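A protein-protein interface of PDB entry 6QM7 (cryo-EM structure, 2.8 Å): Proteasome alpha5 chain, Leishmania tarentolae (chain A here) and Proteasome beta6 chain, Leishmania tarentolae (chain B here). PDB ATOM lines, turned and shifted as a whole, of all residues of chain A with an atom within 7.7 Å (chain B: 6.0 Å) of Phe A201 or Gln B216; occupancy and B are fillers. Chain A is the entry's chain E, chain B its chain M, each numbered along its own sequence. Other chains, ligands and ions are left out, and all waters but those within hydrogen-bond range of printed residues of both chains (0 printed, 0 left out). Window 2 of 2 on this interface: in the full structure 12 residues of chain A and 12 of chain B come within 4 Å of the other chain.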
ATOM      1  N   VAL A 194      10.277   4.483  10.433  1.00  0.00           N
ATOM      2  CA  VAL A 194      11.386   4.038   9.554  1.00  0.00           C
ATOM      3  C   VAL A 194      12.324   3.143  10.361  1.00  0.00           C
ATOM      4  O   VAL A 194      12.738   2.105   9.816  1.00  0.00           O
ATOM      5  CB  VAL A 194      12.083   5.236   8.902  1.00  0.00           C
ATOM      6  CG1 VAL A 194      13.472   4.895   8.391  1.00  0.00           C
ATOM      7  CG2 VAL A 194      11.219   5.768   7.776  1.00  0.00           C
ATOM      8  N   GLU A 195      12.615   3.504  11.607  1.00  0.00           N
ATOM      9  CA  GLU A 195      13.546   2.735  12.471  1.00  0.00           C
ATOM     10  C   GLU A 195      12.886   1.418  12.888  1.00  0.00           C
ATOM     11  O   GLU A 195      13.568   0.388  12.813  1.00  0.00           O
ATOM     12  CB  GLU A 195      14.006   3.594  13.650  1.00  0.00           C
ATOM     13  CG  GLU A 195      14.875   4.767  13.207  1.00  0.00           C
ATOM     14  CD  GLU A 195      16.270   4.412  12.684  1.00  0.00           C
ATOM     15  OE1 GLU A 195      17.259   4.677  13.415  1.00  0.00           O
ATOM     16  OE2 GLU A 195      16.374   3.893  11.540  1.00  0.00           O
ATOM     17  N   SER A 196      11.617   1.460  13.295  1.00  0.00           N
ATOM     18  CA  SER A 196      10.801   0.281  13.679  1.00  0.00           C
ATOM     19  C   SER A 196      10.839  -0.755  12.564  1.00  0.00           C
ATOM     20  O   SER A 196      10.950  -1.938  12.876  1.00  0.00           O
ATOM     21  CB  SER A 196       9.390   0.671  13.993  1.00  0.00           C
ATOM     22  OG  SER A 196       9.316   1.242  15.291  1.00  0.00           O
ATOM     23  N   GLN A 197      10.712  -0.308  11.319  1.00  0.00           N
ATOM     24  CA  GLN A 197      10.564  -1.191  10.143  1.00  0.00           C
ATOM     25  C   GLN A 197      11.946  -1.665   9.712  1.00  0.00           C
ATOM     26  O   GLN A 197      12.043  -2.826   9.255  1.00  0.00           O
ATOM     27  CB  GLN A 197       9.803  -0.487   9.013  1.00  0.00           C
ATOM     28  CG  GLN A 197       8.295  -0.398   9.244  1.00  0.00           C
ATOM     29  CD  GLN A 197       7.662  -1.723   9.610  1.00  0.00           C
ATOM     30  OE1 GLN A 197       7.742  -2.694   8.850  1.00  0.00           O
ATOM     31  NE2 GLN A 197       7.065  -1.782  10.795  1.00  0.00           N
ATOM     32  N   ASN A 198      12.957  -0.802   9.829  1.00  0.00           N
ATOM     33  CA  ASN A 198      14.379  -1.191   9.669  1.00  0.00           C
ATOM     34  C   ASN A 198      14.727  -2.280  10.681  1.00  0.00           C
ATOM     35  O   ASN A 198      15.480  -3.184  10.314  1.00  0.00           O
ATOM     36  CB  ASN A 198      15.334  -0.011   9.806  1.00  0.00           C
ATOM     37  CG  ASN A 198      15.481   0.743   8.504  1.00  0.00           C
ATOM     38  OD1 ASN A 198      15.532   0.130   7.435  1.00  0.00           O
ATOM     39  ND2 ASN A 198      15.563   2.067   8.583  1.00  0.00           N
ATOM     40  N   HIS A 199      14.216  -2.200  11.903  1.00  0.00           N
ATOM     41  CA  HIS A 199      14.470  -3.225  12.938  1.00  0.00           C
ATOM     42  C   HIS A 199      13.857  -4.539  12.484  1.00  0.00           C
ATOM     43  O   HIS A 199      14.588  -5.529  12.455  1.00  0.00           O
ATOM     44  CB  HIS A 199      13.939  -2.811  14.314  1.00  0.00           C
ATOM     45  CG  HIS A 199      14.534  -3.631  15.398  1.00  0.00           C
ATOM     46  ND1 HIS A 199      15.710  -3.272  16.017  1.00  0.00           N
ATOM     47  CD2 HIS A 199      14.173  -4.830  15.906  1.00  0.00           C
ATOM     48  CE1 HIS A 199      16.023  -4.200  16.904  1.00  0.00           C
ATOM     49  NE2 HIS A 199      15.092  -5.165  16.862  1.00  0.00           N
ATOM     50  N   ARG A 200      12.566  -4.530  12.138  1.00  0.00           N
ATOM     51  CA  ARG A 200      11.845  -5.711  11.586  1.00  0.00           C
ATOM     52  C   ARG A 200      12.612  -6.259  10.392  1.00  0.00           C
ATOM     53  O   ARG A 200      12.838  -7.447  10.344  1.00  0.00           O
ATOM     54  CB  ARG A 200      10.424  -5.370  11.138  1.00  0.00           C
ATOM     55  CG  ARG A 200       9.440  -5.370  12.291  1.00  0.00           C
ATOM     56  CD  ARG A 200       8.008  -5.395  11.820  1.00  0.00           C
ATOM     57  NE  ARG A 200       7.117  -5.173  12.950  1.00  0.00           N
ATOM     58  CZ  ARG A 200       6.686  -6.114  13.788  1.00  0.00           C
ATOM     59  NH1 ARG A 200       7.057  -7.379  13.635  1.00  0.00           N
ATOM     60  NH2 ARG A 200       5.866  -5.772  14.775  1.00  0.00           N
ATOM     61  N   PHE A 201      12.971  -5.398   9.456  1.00  0.00           N
ATOM     62  CA  PHE A 201      13.725  -5.795   8.250  1.00  0.00           C
ATOM     63  C   PHE A 201      14.954  -6.601   8.647  1.00  0.00           C
ATOM     64  O   PHE A 201      15.175  -7.693   8.103  1.00  0.00           O
ATOM     65  CB  PHE A 201      14.195  -4.581   7.462  1.00  0.00           C
ATOM     66  CG  PHE A 201      14.842  -5.005   6.183  1.00  0.00           C
ATOM     67  CD1 PHE A 201      14.066  -5.482   5.141  1.00  0.00           C
ATOM     68  CD2 PHE A 201      16.220  -4.997   6.046  1.00  0.00           C
ATOM     69  CE1 PHE A 201      14.661  -5.918   3.971  1.00  0.00           C
ATOM     70  CE2 PHE A 201      16.810  -5.411   4.861  1.00  0.00           C
ATOM     71  CZ  PHE A 201      16.029  -5.887   3.836  1.00  0.00           C
ATOM     72  N   THR A 202      15.734  -6.046   9.566  1.00  0.00           N
ATOM     73  CA  THR A 202      17.108  -6.499   9.884  1.00  0.00           C
ATOM     74  C   THR A 202      17.064  -7.670  10.865  1.00  0.00           C
ATOM     75  O   THR A 202      17.858  -8.576  10.664  1.00  0.00           O
ATOM     76  CB  THR A 202      17.961  -5.343  10.404  1.00  0.00           C
ATOM     77  OG1 THR A 202      18.071  -4.364   9.371  1.00  0.00           O
ATOM     78  CG2 THR A 202      19.340  -5.803  10.808  1.00  0.00           C
ATOM     79  N   TYR A 203      16.168  -7.672  11.851  1.00  0.00           N
ATOM     80  CA  TYR A 203      16.149  -8.669  12.950  1.00  0.00           C
ATOM     81  C   TYR A 203      14.873  -9.521  12.952  1.00  0.00           C
ATOM     82  O   TYR A 203      14.696 -10.315  13.877  1.00  0.00           O
ATOM     83  CB  TYR A 203      16.318  -7.937  14.278  1.00  0.00           C
ATOM     84  CG  TYR A 203      17.594  -7.138  14.379  1.00  0.00           C
ATOM     85  CD1 TYR A 203      18.809  -7.751  14.638  1.00  0.00           C
ATOM     86  CD2 TYR A 203      17.586  -5.763  14.231  1.00  0.00           C
ATOM     87  CE1 TYR A 203      19.982  -7.020  14.742  1.00  0.00           C
ATOM     88  CE2 TYR A 203      18.748  -5.014  14.335  1.00  0.00           C
ATOM     89  CZ  TYR A 203      19.951  -5.644  14.588  1.00  0.00           C
ATOM     90  OH  TYR A 203      21.093  -4.900  14.698  1.00  0.00           O
ATOM     91  N   ASN A 204      14.004  -9.381  11.961  1.00  0.00           N
ATOM     92  CA  ASN A 204      12.768 -10.194  11.818  1.00  0.00           C
ATOM     93  C   ASN A 204      12.017 -10.237  13.133  1.00  0.00           C
ATOM     94  O   ASN A 204      11.583 -11.323  13.533  1.00  0.00           O
ATOM     95  CB  ASN A 204      13.074 -11.623  11.374  1.00  0.00           C
ATOM     96  CG  ASN A 204      11.875 -12.377  10.842  1.00  0.00           C
ATOM     97  OD1 ASN A 204      10.820 -11.799  10.568  1.00  0.00           O
ATOM     98  ND2 ASN A 204      12.040 -13.681  10.708  1.00  0.00           N
ATOM     99  N   GLU A 205      11.888  -9.104  13.796  1.00  0.00           N
ATOM    100  CA  GLU A 205      11.178  -9.061  15.088  1.00  0.00           C
ATOM    101  C   GLU A 205      10.713  -7.646  15.334  1.00  0.00           C
ATOM    102  O   GLU A 205      11.329  -6.709  14.841  1.00  0.00           O
ATOM    103  CB  GLU A 205      12.077  -9.550  16.226  1.00  0.00           C
ATOM    104  CG  GLU A 205      13.198  -8.593  16.579  1.00  0.00           C
ATOM    105  CD  GLU A 205      14.167  -9.122  17.620  1.00  0.00           C
ATOM    106  OE1 GLU A 205      14.129 -10.350  17.909  1.00  0.00           O
ATOM    107  OE2 GLU A 205      14.939  -8.300  18.154  1.00  0.00           O
ATOM    108  N   THR B 211      18.086 -16.210  18.380  1.00  0.00           N
ATOM    109  CA  THR B 211      18.764 -16.927  17.283  1.00  0.00           C
ATOM    110  C   THR B 211      18.139 -16.475  15.973  1.00  0.00           C
ATOM    111  O   THR B 211      18.872 -16.377  14.982  1.00  0.00           O
ATOM    112  CB  THR B 211      18.630 -18.437  17.457  1.00  0.00           C
ATOM    113  OG1 THR B 211      19.363 -18.752  18.642  1.00  0.00           O
ATOM    114  CG2 THR B 211      19.130 -19.216  16.259  1.00  0.00           C
ATOM    115  N   LYS B 212      16.828 -16.240  15.997  1.00  0.00           N
ATOM    116  CA  LYS B 212      16.012 -15.870  14.815  1.00  0.00           C
ATOM    117  C   LYS B 212      16.444 -14.491  14.323  1.00  0.00           C
ATOM    118  O   LYS B 212      16.525 -14.292  13.106  1.00  0.00           O
ATOM    119  CB  LYS B 212      14.523 -15.869  15.177  1.00  0.00           C
ATOM    120  CG  LYS B 212      13.578 -16.022  13.993  1.00  0.00           C
ATOM    121  CD  LYS B 212      12.484 -14.976  13.930  1.00  0.00           C
ATOM    122  CE  LYS B 212      11.355 -15.233  14.905  1.00  0.00           C
ATOM    123  NZ  LYS B 212      10.661 -13.968  15.260  1.00  0.00           N
ATOM    124  N   ALA B 213      16.681 -13.573  15.254  1.00  0.00           N
ATOM    125  CA  ALA B 213      17.121 -12.187  14.989  1.00  0.00           C
ATOM    126  C   ALA B 213      18.514 -12.196  14.362  1.00  0.00           C
ATOM    127  O   ALA B 213      18.764 -11.409  13.421  1.00  0.00           O
ATOM    128  CB  ALA B 213      17.130 -11.393  16.268  1.00  0.00           C
ATOM    129  N   ILE B 214      19.393 -13.029  14.899  1.00  0.00           N
ATOM    130  CA  ILE B 214      20.796 -13.144  14.438  1.00  0.00           C
ATOM    131  C   ILE B 214      20.823 -13.787  13.062  1.00  0.00           C
ATOM    132  O   ILE B 214      21.736 -13.488  12.287  1.00  0.00           O
ATOM    133  CB  ILE B 214      21.604 -13.940  15.461  1.00  0.00           C
ATOM    134  CG1 ILE B 214      21.841 -13.072  16.693  1.00  0.00           C
ATOM    135  CG2 ILE B 214      22.900 -14.445  14.860  1.00  0.00           C
ATOM    136  CD1 ILE B 214      22.521 -13.800  17.805  1.00  0.00           C
ATOM    137  N   ALA B 215      19.883 -14.679  12.806  1.00  0.00           N
ATOM    138  CA  ALA B 215      19.752 -15.351  11.509  1.00  0.00           C
ATOM    139  C   ALA B 215      19.324 -14.324  10.458  1.00  0.00           C
ATOM    140  O   ALA B 215      19.821 -14.417   9.298  1.00  0.00           O
ATOM    141  CB  ALA B 215      18.773 -16.486  11.617  1.00  0.00           C
ATOM    142  N   GLN B 216      18.428 -13.392  10.802  1.00  0.00           N
ATOM    143  CA  GLN B 216      17.988 -12.375   9.809  1.00  0.00           C
ATOM    144  C   GLN B 216      19.131 -11.389   9.641  1.00  0.00           C
ATOM    145  O   GLN B 216      19.399 -10.984   8.505  1.00  0.00           O
ATOM    146  CB  GLN B 216      16.689 -11.656  10.174  1.00  0.00           C
ATOM    147  CG  GLN B 216      15.603 -11.811   9.114  1.00  0.00           C
ATOM    148  CD  GLN B 216      16.018 -11.386   7.732  1.00  0.00           C
ATOM    149  OE1 GLN B 216      15.675 -12.036   6.744  1.00  0.00           O
ATOM    150  NE2 GLN B 216      16.724 -10.267   7.654  1.00  0.00           N
ATOM    151  N   LEU B 217      19.797 -11.053  10.737  1.00  0.00           N
ATOM    152  CA  LEU B 217      20.941 -10.119  10.715  1.00  0.00           C
ATOM    153  C   LEU B 217      22.009 -10.676   9.786  1.00  0.00           C
ATOM    154  O   LEU B 217      22.557  -9.900   9.027  1.00  0.00           O
ATOM    155  CB  LEU B 217      21.481  -9.968  12.132  1.00  0.00           C
ATOM    156  CG  LEU B 217      22.721  -9.096  12.247  1.00  0.00           C
ATOM    157  CD1 LEU B 217      22.420  -7.684  11.788  1.00  0.00           C
ATOM    158  CD2 LEU B 217      23.228  -9.111  13.674  1.00  0.00           C
ATOM    159  N   MET B 218      22.283 -11.971   9.869  1.00  0.00           N
ATOM    160  CA  MET B 218      23.312 -12.651   9.052  1.00  0.00           C
ATOM    161  C   MET B 218      22.901 -12.607   7.571  1.00  0.00           C
ATOM    162  O   MET B 218      23.766 -12.320   6.751  1.00  0.00           O
ATOM    163  CB  MET B 218      23.484 -14.092   9.540  1.00  0.00           C
ATOM    164  CG  MET B 218      24.371 -14.967   8.676  1.00  0.00           C
ATOM    165  SD  MET B 218      26.092 -14.487   8.802  1.00  0.00           S
ATOM    166  CE  MET B 218      26.543 -15.550  10.168  1.00  0.00           C
ATOM    167  N   SER B 219      21.631 -12.868   7.241  1.00  0.00           N
ATOM    168  CA  SER B 219      21.076 -12.745   5.859  1.00  0.00           C
ATOM    169  C   SER B 219      21.360 -11.347   5.330  1.00  0.00           C
ATOM    170  O   SER B 219      21.791 -11.216   4.169  1.00  0.00           O
ATOM    171  CB  SER B 219      19.587 -12.998   5.786  1.00  0.00           C
ATOM    172  OG  SER B 219      19.310 -14.342   5.426  1.00  0.00           O
ATOM    173  N   THR B 220      21.067 -10.357   6.171  1.00  0.00           N
ATOM    174  CA  THR B 220      21.064  -8.922   5.828  1.00  0.00           C
ATOM    175  C   THR B 220      22.501  -8.472   5.623  1.00  0.00           C
ATOM    176  O   THR B 220      22.745  -7.775   4.640  1.00  0.00           O
ATOM    177  CB  THR B 220      20.348  -8.114   6.912  1.00  0.00           C
ATOM    178  OG1 THR B 220      18.965  -8.479   6.922  1.00  0.00           O
ATOM    179  CG2 THR B 220      20.471  -6.623   6.694  1.00  0.00           C
ATOM    180  N   MET B 221      23.411  -8.879   6.500  1.00  0.00           N
ATOM    181  CA  MET B 221      24.830  -8.452   6.468  1.00  0.00           C
ATOM    182  C   MET B 221      25.541  -9.079   5.276  1.00  0.00           C
ATOM    183  O   MET B 221      26.372  -8.371   4.666  1.00  0.00           O
ATOM    184  CB  MET B 221      25.554  -8.861   7.744  1.00  0.00           C
ATOM    185  CG  MET B 221      25.095  -8.060   8.939  1.00  0.00           C
ATOM    186  SD  MET B 221      26.135  -8.387  10.355  1.00  0.00           S
ATOM    187  CE  MET B 221      27.574  -7.465   9.817  1.00  0.00           C
ATOM    188  N   HIS B 224      24.316  -7.232   2.099  1.00  0.00           N
ATOM    189  CA  HIS B 224      24.887  -5.866   2.000  1.00  0.00           C
ATOM    190  C   HIS B 224      26.274  -5.927   1.368  1.00  0.00           C
ATOM    191  O   HIS B 224      26.754  -4.869   0.942  1.00  0.00           O
ATOM    192  CB  HIS B 224      24.900  -5.143   3.356  1.00  0.00           C
ATOM    193  CG  HIS B 224      23.546  -4.679   3.781  1.00  0.00           C
ATOM    194  ND1 HIS B 224      23.279  -4.280   5.077  1.00  0.00           N
ATOM    195  CD2 HIS B 224      22.380  -4.583   3.099  1.00  0.00           C
ATOM    196  CE1 HIS B 224      22.012  -3.930   5.170  1.00  0.00           C
ATOM    197  NE2 HIS B 224      21.437  -4.116   3.972  1.00  0.00           N
ATOM    198  N   TYR B 250      23.297 -20.798   5.279  1.00  0.00           N
ATOM    199  CA  TYR B 250      23.290 -19.675   4.312  1.00  0.00           C
ATOM    200  C   TYR B 250      24.031 -20.063   3.043  1.00  0.00           C
ATOM    201  O   TYR B 250      24.861 -20.975   3.076  1.00  0.00           O
ATOM    202  CB  TYR B 250      23.939 -18.448   4.946  1.00  0.00           C
ATOM    203  CG  TYR B 250      23.155 -17.938   6.117  1.00  0.00           C
ATOM    204  CD1 TYR B 250      22.310 -16.856   6.000  1.00  0.00           C
ATOM    205  CD2 TYR B 250      23.218 -18.579   7.328  1.00  0.00           C
ATOM    206  CE1 TYR B 250      21.569 -16.398   7.074  1.00  0.00           C
ATOM    207  CE2 TYR B 250      22.490 -18.132   8.421  1.00  0.00           C
ATOM    208  CZ  TYR B 250      21.657 -17.040   8.292  1.00  0.00           C
ATOM    209  OH  TYR B 250      20.934 -16.636   9.363  1.00  0.00           O
ATOM    210  N   THR B 256      18.627 -18.132   3.263  1.00  0.00           N
ATOM    211  CA  THR B 256      18.590 -19.114   4.367  1.00  0.00           C
ATOM    212  C   THR B 256      17.166 -19.618   4.554  1.00  0.00           C
ATOM    213  O   THR B 256      16.229 -19.051   3.964  1.00  0.00           O
ATOM    214  CB  THR B 256      19.132 -18.497   5.666  1.00  0.00           C
ATOM    215  OG1 THR B 256      19.272 -19.546   6.621  1.00  0.00           O
ATOM    216  CG2 THR B 256      18.259 -17.401   6.249  1.00  0.00           C
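NE2 of Gln B216 sits at hydrogen-bond distance from OG1 of Thr B220, 3.0 Å away.
The backbone carbonyl oxygen (O) of Asn A198 lies within hydrogen-bond range of the side-chain hydroxyl (OG1) of Thr A202, at 3.0 Å.
NE2 of His A199 lies within hydrogen-bond range of OE2 of Glu A205.
The backbone NH (N) of Leu B217 is in hydrogen-bond range of the backbone carbonyl oxygen (O) of Thr A202 (3.1 Å).
The side-chain amino group (NZ) of Lys B212 is in hydrogen-bond range of the backbone carbonyl oxygen (O) of Asn A204 (3.3 Å).
The backbone carbonyl oxygen (O) of Phe A201 lies within hydrogen-bond range of the side-chain amide nitrogen (NE2) of Gln B216, at 3.0 Å.
Of the printed residues of chain B, Phe A201 touches Gln B216.
Gln B216 touches just these residues of chain A: Phe A201 (3.0 Å), Thr A202 (3.3 Å), Tyr A203 (3.9 Å) and Asn A204 (3.4 Å).
Of the printed residues of chain A, Ala B213 touches Tyr A203 and Glu A205.
Printed residues of chain B within 4 Å of Tyr A203: Ala B213 (3.3 Å), Gln B216 (3.9 Å) and Leu B217 (3.9 Å).
Of the printed residues of chain B, Glu A205 touches Ala B213.
The nearest printed residue of chain A that does not touch Lys B212 is Tyr A203 (4.4 Å).
Thr A202 touches Gln B216.
O of Thr A202 touches OG1 of Thr B220 (3.9 Å).
Tyr A203 touches Ala B213.
Tyr A203 touches Gln B216 (C to CB, 3.9 Å).
Tyr A203 touches Leu B217 (CE1 to CD1, 3.9 Å).
Gln B216 touches Asn A204.
Glu A205 touches Ala B213 (OE1 to CB, 3.6 Å).
Hydrophobic or aromatic side chains of chain B that line the printed part of chain A: Ala B213 and Leu B217.
Along chain A the printed residues that touch a printed residue of chain B span positions 201 to 205.
Among the printed residues, no Asp or Glu carboxylate lies within 4 Å of a Lys or Arg side-chain nitrogen of the other chain.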
